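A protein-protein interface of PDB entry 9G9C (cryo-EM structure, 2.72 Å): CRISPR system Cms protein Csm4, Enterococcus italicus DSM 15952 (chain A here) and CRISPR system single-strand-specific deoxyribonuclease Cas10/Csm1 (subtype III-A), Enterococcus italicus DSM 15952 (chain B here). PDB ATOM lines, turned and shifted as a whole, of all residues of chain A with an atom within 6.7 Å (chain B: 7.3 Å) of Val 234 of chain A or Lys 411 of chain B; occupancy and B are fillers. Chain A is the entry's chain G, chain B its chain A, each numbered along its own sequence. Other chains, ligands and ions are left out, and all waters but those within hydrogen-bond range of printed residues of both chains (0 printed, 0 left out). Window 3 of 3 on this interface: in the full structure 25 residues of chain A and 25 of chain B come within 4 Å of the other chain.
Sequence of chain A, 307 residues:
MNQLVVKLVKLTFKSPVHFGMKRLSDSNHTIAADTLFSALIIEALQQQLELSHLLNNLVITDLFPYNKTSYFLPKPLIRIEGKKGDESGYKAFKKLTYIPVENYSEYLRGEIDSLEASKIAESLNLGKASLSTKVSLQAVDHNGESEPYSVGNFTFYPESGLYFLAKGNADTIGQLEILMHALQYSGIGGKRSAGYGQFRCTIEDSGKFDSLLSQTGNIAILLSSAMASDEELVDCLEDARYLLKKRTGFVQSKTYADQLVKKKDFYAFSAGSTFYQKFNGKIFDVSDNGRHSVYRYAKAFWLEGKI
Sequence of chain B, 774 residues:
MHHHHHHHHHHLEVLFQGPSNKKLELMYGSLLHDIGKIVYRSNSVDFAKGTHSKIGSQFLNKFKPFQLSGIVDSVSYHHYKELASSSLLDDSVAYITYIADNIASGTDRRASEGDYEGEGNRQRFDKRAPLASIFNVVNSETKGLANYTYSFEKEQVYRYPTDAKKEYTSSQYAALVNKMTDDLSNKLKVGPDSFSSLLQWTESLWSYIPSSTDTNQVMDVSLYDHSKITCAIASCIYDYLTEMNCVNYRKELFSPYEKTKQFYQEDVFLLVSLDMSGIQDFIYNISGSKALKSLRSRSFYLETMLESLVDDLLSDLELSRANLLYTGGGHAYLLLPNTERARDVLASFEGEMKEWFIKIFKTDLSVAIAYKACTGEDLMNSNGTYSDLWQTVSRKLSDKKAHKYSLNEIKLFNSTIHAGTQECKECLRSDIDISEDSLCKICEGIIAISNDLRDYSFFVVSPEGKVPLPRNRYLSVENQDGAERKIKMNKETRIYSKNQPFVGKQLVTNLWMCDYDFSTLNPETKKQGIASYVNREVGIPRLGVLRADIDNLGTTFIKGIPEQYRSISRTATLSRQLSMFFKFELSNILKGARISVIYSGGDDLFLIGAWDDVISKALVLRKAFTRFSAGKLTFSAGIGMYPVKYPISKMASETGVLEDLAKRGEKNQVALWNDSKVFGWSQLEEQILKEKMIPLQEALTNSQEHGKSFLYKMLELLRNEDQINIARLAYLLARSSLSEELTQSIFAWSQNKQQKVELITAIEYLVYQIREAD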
ATOM      1  N   ALA A 228     -23.389   2.848  22.809  1.00  0.00           N
ATOM      2  CA  ALA A 228     -22.954   3.973  21.951  1.00  0.00           C
ATOM      3  C   ALA A 228     -22.117   3.495  20.771  1.00  0.00           C
ATOM      4  O   ALA A 228     -21.574   2.373  20.815  1.00  0.00           O
ATOM      5  CB  ALA A 228     -22.143   4.927  22.787  1.00  0.00           C
ATOM      6  N   SER A 229     -22.020   4.311  19.722  1.00  0.00           N
ATOM      7  CA  SER A 229     -21.112   3.944  18.609  1.00  0.00           C
ATOM      8  C   SER A 229     -19.677   4.116  19.120  1.00  0.00           C
ATOM      9  O   SER A 229     -19.504   4.767  20.168  1.00  0.00           O
ATOM     10  CB  SER A 229     -21.368   4.766  17.383  1.00  0.00           C
ATOM     11  OG  SER A 229     -20.956   6.108  17.590  1.00  0.00           O
ATOM     12  N   ASP A 230     -18.693   3.544  18.428  1.00  0.00           N
ATOM     13  CA  ASP A 230     -17.289   3.595  18.922  1.00  0.00           C
ATOM     14  C   ASP A 230     -16.886   5.045  19.213  1.00  0.00           C
ATOM     15  O   ASP A 230     -16.364   5.303  20.315  1.00  0.00           O
ATOM     16  CB  ASP A 230     -16.351   2.888  17.958  1.00  0.00           C
ATOM     17  CG  ASP A 230     -16.456   1.370  17.972  1.00  0.00           C
ATOM     18  OD1 ASP A 230     -17.283   0.850  18.750  1.00  0.00           O
ATOM     19  OD2 ASP A 230     -15.708   0.723  17.210  1.00  0.00           O
ATOM     20  N   GLU A 231     -17.119   5.951  18.263  1.00  0.00           N
ATOM     21  CA  GLU A 231     -16.736   7.374  18.448  1.00  0.00           C
ATOM     22  C   GLU A 231     -17.528   7.968  19.623  1.00  0.00           C
ATOM     23  O   GLU A 231     -16.923   8.710  20.419  1.00  0.00           O
ATOM     24  CB  GLU A 231     -16.957   8.149  17.149  1.00  0.00           C
ATOM     25  CG  GLU A 231     -18.351   7.984  16.550  1.00  0.00           C
ATOM     26  CD  GLU A 231     -18.534   6.838  15.569  1.00  0.00           C
ATOM     27  OE1 GLU A 231     -18.879   7.122  14.403  1.00  0.00           O
ATOM     28  OE2 GLU A 231     -18.342   5.667  15.961  1.00  0.00           O
ATOM     29  N   GLU A 232     -18.815   7.643  19.735  1.00  0.00           N
ATOM     30  CA  GLU A 232     -19.654   8.118  20.868  1.00  0.00           C
ATOM     31  C   GLU A 232     -19.109   7.544  22.181  1.00  0.00           C
ATOM     32  O   GLU A 232     -19.136   8.262  23.200  1.00  0.00           O
ATOM     33  CB  GLU A 232     -21.123   7.755  20.660  1.00  0.00           C
ATOM     34  CG  GLU A 232     -21.780   8.581  19.560  1.00  0.00           C
ATOM     35  CD  GLU A 232     -23.199   8.145  19.258  1.00  0.00           C
ATOM     36  OE1 GLU A 232     -23.385   6.967  18.895  1.00  0.00           O
ATOM     37  OE2 GLU A 232     -24.111   8.988  19.382  1.00  0.00           O
ATOM     38  N   LEU A 233     -18.648   6.292  22.151  1.00  0.00           N
ATOM     39  CA  LEU A 233     -18.217   5.607  23.399  1.00  0.00           C
ATOM     40  C   LEU A 233     -17.072   6.365  24.075  1.00  0.00           C
ATOM     41  O   LEU A 233     -17.094   6.468  25.318  1.00  0.00           O
ATOM     42  CB  LEU A 233     -17.807   4.163  23.103  1.00  0.00           C
ATOM     43  CG  LEU A 233     -17.734   3.221  24.305  1.00  0.00           C
ATOM     44  CD1 LEU A 233     -19.104   3.093  24.933  1.00  0.00           C
ATOM     45  CD2 LEU A 233     -17.232   1.858  23.877  1.00  0.00           C
ATOM     46  N   VAL A 234     -16.116   6.880  23.303  1.00  0.00           N
ATOM     47  CA  VAL A 234     -14.942   7.486  23.993  1.00  0.00           C
ATOM     48  C   VAL A 234     -15.344   8.705  24.839  1.00  0.00           C
ATOM     49  O   VAL A 234     -14.901   8.766  26.006  1.00  0.00           O
ATOM     50  CB  VAL A 234     -13.946   7.909  22.899  1.00  0.00           C
ATOM     51  CG1 VAL A 234     -12.594   8.295  23.483  1.00  0.00           C
ATOM     52  CG2 VAL A 234     -13.784   6.835  21.832  1.00  0.00           C
ATOM     53  N   ASP A 235     -16.164   9.621  24.316  1.00  0.00           N
ATOM     54  CA  ASP A 235     -16.663  10.748  25.158  1.00  0.00           C
ATOM     55  C   ASP A 235     -17.596  10.274  26.278  1.00  0.00           C
ATOM     56  O   ASP A 235     -17.479  10.803  27.403  1.00  0.00           O
ATOM     57  CB  ASP A 235     -17.324  11.835  24.325  1.00  0.00           C
ATOM     58  CG  ASP A 235     -18.312  11.354  23.275  1.00  0.00           C
ATOM     59  OD1 ASP A 235     -17.862  10.721  22.300  1.00  0.00           O
ATOM     60  OD2 ASP A 235     -19.525  11.603  23.451  1.00  0.00           O
ATOM     61  N   CYS A 236     -18.498   9.334  25.983  1.00  0.00           N
ATOM     62  CA  CYS A 236     -19.552   8.930  26.958  1.00  0.00           C
ATOM     63  C   CYS A 236     -19.023   8.275  28.245  1.00  0.00           C
ATOM     64  O   CYS A 236     -19.567   8.602  29.319  1.00  0.00           O
ATOM     65  CB  CYS A 236     -20.560   8.003  26.287  1.00  0.00           C
ATOM     66  SG  CYS A 236     -20.168   6.243  26.444  1.00  0.00           S
ATOM     67  N   LEU A 237     -18.011   7.412  28.161  1.00  0.00           N
ATOM     68  CA  LEU A 237     -17.594   6.622  29.355  1.00  0.00           C
ATOM     69  C   LEU A 237     -17.092   7.514  30.504  1.00  0.00           C
ATOM     70  O   LEU A 237     -17.368   7.176  31.665  1.00  0.00           O
ATOM     71  CB  LEU A 237     -16.579   5.557  28.951  1.00  0.00           C
ATOM     72  CG  LEU A 237     -17.194   4.224  28.518  1.00  0.00           C
ATOM     73  CD1 LEU A 237     -16.246   3.097  28.843  1.00  0.00           C
ATOM     74  CD2 LEU A 237     -18.509   4.030  29.250  1.00  0.00           C
ATOM     75  N   GLU A 238     -16.340   8.569  30.202  1.00  0.00           N
ATOM     76  CA  GLU A 238     -15.776   9.433  31.271  1.00  0.00           C
ATOM     77  C   GLU A 238     -16.815   9.712  32.372  1.00  0.00           C
ATOM     78  O   GLU A 238     -17.877  10.277  32.028  1.00  0.00           O
ATOM     79  CB  GLU A 238     -15.312  10.745  30.645  1.00  0.00           C
ATOM     80  CG  GLU A 238     -14.837  11.780  31.661  1.00  0.00           C
ATOM     81  CD  GLU A 238     -15.767  12.973  31.791  1.00  0.00           C
ATOM     82  OE1 GLU A 238     -16.816  12.984  31.114  1.00  0.00           O
ATOM     83  OE2 GLU A 238     -15.437  13.897  32.562  1.00  0.00           O
ATOM     84  N   SER B 406     -13.211  -0.316  30.735  1.00  0.00           N
ATOM     85  CA  SER B 406     -12.747   0.816  29.889  1.00  0.00           C
ATOM     86  C   SER B 406     -13.347   0.684  28.486  1.00  0.00           C
ATOM     87  O   SER B 406     -13.763  -0.434  28.128  1.00  0.00           O
ATOM     88  CB  SER B 406     -11.251   0.872  29.814  1.00  0.00           C
ATOM     89  OG  SER B 406     -10.769  -0.011  28.811  1.00  0.00           O
ATOM     90  N   LEU B 407     -13.303   1.756  27.694  1.00  0.00           N
ATOM     91  CA  LEU B 407     -13.977   1.712  26.371  1.00  0.00           C
ATOM     92  C   LEU B 407     -13.323   0.628  25.508  1.00  0.00           C
ATOM     93  O   LEU B 407     -14.068  -0.079  24.811  1.00  0.00           O
ATOM     94  CB  LEU B 407     -13.949   3.077  25.685  1.00  0.00           C
ATOM     95  CG  LEU B 407     -12.590   3.776  25.591  1.00  0.00           C
ATOM     96  CD1 LEU B 407     -12.189   3.934  24.136  1.00  0.00           C
ATOM     97  CD2 LEU B 407     -12.670   5.129  26.273  1.00  0.00           C
ATOM     98  N   ASN B 408     -11.999   0.500  25.548  1.00  0.00           N
ATOM     99  CA  ASN B 408     -11.353  -0.484  24.641  1.00  0.00           C
ATOM    100  C   ASN B 408     -11.839  -1.891  24.997  1.00  0.00           C
ATOM    101  O   ASN B 408     -12.138  -2.662  24.067  1.00  0.00           O
ATOM    102  CB  ASN B 408      -9.832  -0.401  24.697  1.00  0.00           C
ATOM    103  CG  ASN B 408      -9.308   0.989  24.419  1.00  0.00           C
ATOM    104  OD1 ASN B 408      -8.787   1.245  23.329  1.00  0.00           O
ATOM    105  ND2 ASN B 408      -9.444   1.897  25.374  1.00  0.00           N
ATOM    106  N   GLU B 409     -11.934  -2.207  26.291  1.00  0.00           N
ATOM    107  CA  GLU B 409     -12.478  -3.527  26.709  1.00  0.00           C
ATOM    108  C   GLU B 409     -13.949  -3.643  26.281  1.00  0.00           C
ATOM    109  O   GLU B 409     -14.337  -4.724  25.801  1.00  0.00           O
ATOM    110  CB  GLU B 409     -12.319  -3.702  28.217  1.00  0.00           C
ATOM    111  CG  GLU B 409     -10.941  -3.280  28.720  1.00  0.00           C
ATOM    112  CD  GLU B 409     -10.803  -3.183  30.228  1.00  0.00           C
ATOM    113  OE1 GLU B 409     -11.580  -2.428  30.845  1.00  0.00           O
ATOM    114  OE2 GLU B 409      -9.907  -3.853  30.784  1.00  0.00           O
ATOM    115  N   ILE B 410     -14.729  -2.569  26.448  1.00  0.00           N
ATOM    116  CA  ILE B 410     -16.174  -2.591  26.067  1.00  0.00           C
ATOM    117  C   ILE B 410     -16.283  -2.806  24.552  1.00  0.00           C
ATOM    118  O   ILE B 410     -17.107  -3.643  24.127  1.00  0.00           O
ATOM    119  CB  ILE B 410     -16.875  -1.293  26.509  1.00  0.00           C
ATOM    120  CG1 ILE B 410     -16.863  -1.148  28.023  1.00  0.00           C
ATOM    121  CG2 ILE B 410     -18.297  -1.212  25.954  1.00  0.00           C
ATOM    122  CD1 ILE B 410     -17.795  -0.073  28.549  1.00  0.00           C
ATOM    123  N   LYS B 411     -15.433  -2.129  23.780  1.00  0.00           N
ATOM    124  CA  LYS B 411     -15.438  -2.306  22.309  1.00  0.00           C
ATOM    125  C   LYS B 411     -15.056  -3.753  21.990  1.00  0.00           C
ATOM    126  O   LYS B 411     -15.671  -4.341  21.083  1.00  0.00           O
ATOM    127  CB  LYS B 411     -14.468  -1.314  21.661  1.00  0.00           C
ATOM    128  CG  LYS B 411     -14.948   0.127  21.696  1.00  0.00           C
ATOM    129  CD  LYS B 411     -13.968   1.149  21.136  1.00  0.00           C
ATOM    130  CE  LYS B 411     -14.471   2.541  21.335  1.00  0.00           C
ATOM    131  NZ  LYS B 411     -13.623   3.529  20.664  1.00  0.00           N
ATOM    132  N   LEU B 412     -14.076  -4.296  22.711  1.00  0.00           N
ATOM    133  CA  LEU B 412     -13.607  -5.676  22.434  1.00  0.00           C
ATOM    134  C   LEU B 412     -14.742  -6.678  22.690  1.00  0.00           C
ATOM    135  O   LEU B 412     -14.888  -7.623  21.887  1.00  0.00           O
ATOM    136  CB  LEU B 412     -12.378  -5.995  23.281  1.00  0.00           C
ATOM    137  CG  LEU B 412     -11.058  -6.109  22.512  1.00  0.00           C
ATOM    138  CD1 LEU B 412     -11.157  -7.229  21.493  1.00  0.00           C
ATOM    139  CD2 LEU B 412     -10.725  -4.798  21.827  1.00  0.00           C
ATOM    140  N   PHE B 413     -15.511  -6.478  23.764  1.00  0.00           N
ATOM    141  CA  PHE B 413     -16.642  -7.390  24.052  1.00  0.00           C
ATOM    142  C   PHE B 413     -17.633  -7.298  22.921  1.00  0.00           C
ATOM    143  O   PHE B 413     -18.132  -8.341  22.453  1.00  0.00           O
ATOM    144  CB  PHE B 413     -17.360  -6.819  25.272  1.00  0.00           C
ATOM    145  CG  PHE B 413     -16.723  -6.979  26.643  1.00  0.00           C
ATOM    146  CD1 PHE B 413     -16.001  -8.118  26.976  1.00  0.00           C
ATOM    147  CD2 PHE B 413     -16.867  -5.986  27.604  1.00  0.00           C
ATOM    148  CE1 PHE B 413     -15.438  -8.252  28.234  1.00  0.00           C
ATOM    149  CE2 PHE B 413     -16.295  -6.123  28.857  1.00  0.00           C
ATOM    150  CZ  PHE B 413     -15.584  -7.255  29.169  1.00  0.00           C
ATOM    151  N   ASN B 414     -17.901  -6.075  22.469  1.00  0.00           N
ATOM    152  CA  ASN B 414     -18.845  -5.826  21.343  1.00  0.00           C
ATOM    153  C   ASN B 414     -18.330  -6.422  20.029  1.00  0.00           C
ATOM    154  O   ASN B 414     -19.172  -6.911  19.248  1.00  0.00           O
ATOM    155  CB  ASN B 414     -19.242  -4.356  21.252  1.00  0.00           C
ATOM    156  CG  ASN B 414     -20.160  -3.967  22.384  1.00  0.00           C
ATOM    157  OD1 ASN B 414     -21.191  -4.613  22.591  1.00  0.00           O
ATOM    158  ND2 ASN B 414     -19.797  -2.941  23.137  1.00  0.00           N
ATOM    159  N   SER B 415     -17.020  -6.374  19.767  1.00  0.00           N
ATOM    160  CA  SER B 415     -16.533  -6.764  18.417  1.00  0.00           C
ATOM    161  C   SER B 415     -16.377  -8.278  18.246  1.00  0.00           C
ATOM    162  O   SER B 415     -15.230  -8.733  18.068  1.00  0.00           O
ATOM    163  CB  SER B 415     -15.221  -6.084  18.145  1.00  0.00           C
ATOM    164  OG  SER B 415     -15.266  -4.719  18.535  1.00  0.00           O
ATOM    165  N   THR B 416     -17.486  -9.019  18.260  1.00  0.00           N
ATOM    166  CA  THR B 416     -17.461 -10.461  17.938  1.00  0.00           C
ATOM    167  C   THR B 416     -17.277 -10.584  16.436  1.00  0.00           C
ATOM    168  O   THR B 416     -17.760  -9.682  15.719  1.00  0.00           O
ATOM    169  CB  THR B 416     -18.756 -11.105  18.430  1.00  0.00           C
ATOM    170  OG1 THR B 416     -18.865 -10.742  19.803  1.00  0.00           O
ATOM    171  CG2 THR B 416     -18.760 -12.617  18.298  1.00  0.00           C
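Hydrophobic or aromatic side chains of chain A that line the printed part of chain B: Leu 233, Val 234 and Leu 237.
Printed residues of chain B that touch a printed residue of chain A: Ser 406, Leu 407, Ile 410 and Lys 411.
Hydrophobic or aromatic side chains of chain B within 4 Å of the printed part of chain A: Leu 407 and Ile 410.
The side-chain amino group (NZ) of Lys 411 of chain B lies within hydrogen-bond range of the backbone carbonyl oxygen (O) of Asp 230 of chain A (3.3 Å).
N of Ser 406 of chain B lies within hydrogen-bond range of OE1 of Glu 409 of chain B, at 2.7 Å.
The side-chain amide nitrogen (ND2) of Asn 414 of chain B sits at hydrogen-bond distance from the backbone carbonyl oxygen (O) of Ile 410 of chain B (3.0 Å).
O of Lys 411 of chain B sits at hydrogen-bond distance from OG of Ser 415 of chain B, 2.6 Å away.
O of Leu 233 of chain A lies within hydrogen-bond range of SG of Cys 236 of chain A.
Among the printed residues, merely in contact across the chains: Leu 237 of chain A with Leu 407 of chain B, Val 234 of chain A with Lys 411 of chain B, Leu 237 of chain A with Ile 410 of chain B, Leu 233 of chain A with Lys 411 of chain B, Leu 237 of chain A with Ser 406 of chain B, Leu 233 of chain A with Leu 407 of chain B, Leu 233 of chain A with Ile 410 of chain B and Val 234 of chain A with Leu 407 of chain B.
Printed residues of chain B within 4 Å of Leu 233 of chain A: Leu 407 (3.8 Å), Ile 410 (3.9 Å) and Lys 411 (3.6 Å).
Printed residues of chain B within 4 Å of Val 234 of chain A: Leu 407 and Lys 411.
Of the printed residues of chain B, Leu 237 of chain A touches Ser 406, Leu 407 and Ile 410.
Of the printed residues of chain A, Ser 406 of chain B touches Leu 237.
Of the printed residues of chain A, Ile 410 of chain B touches Leu 233 and Leu 237.
Lys 411 of chain B touches just these residues of chain A: Asp 230, Leu 233 and Val 234.
The nearest printed residue of chain A that does not touch Leu 407 of chain B is Asp 230 of chain A (5.8 Å).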
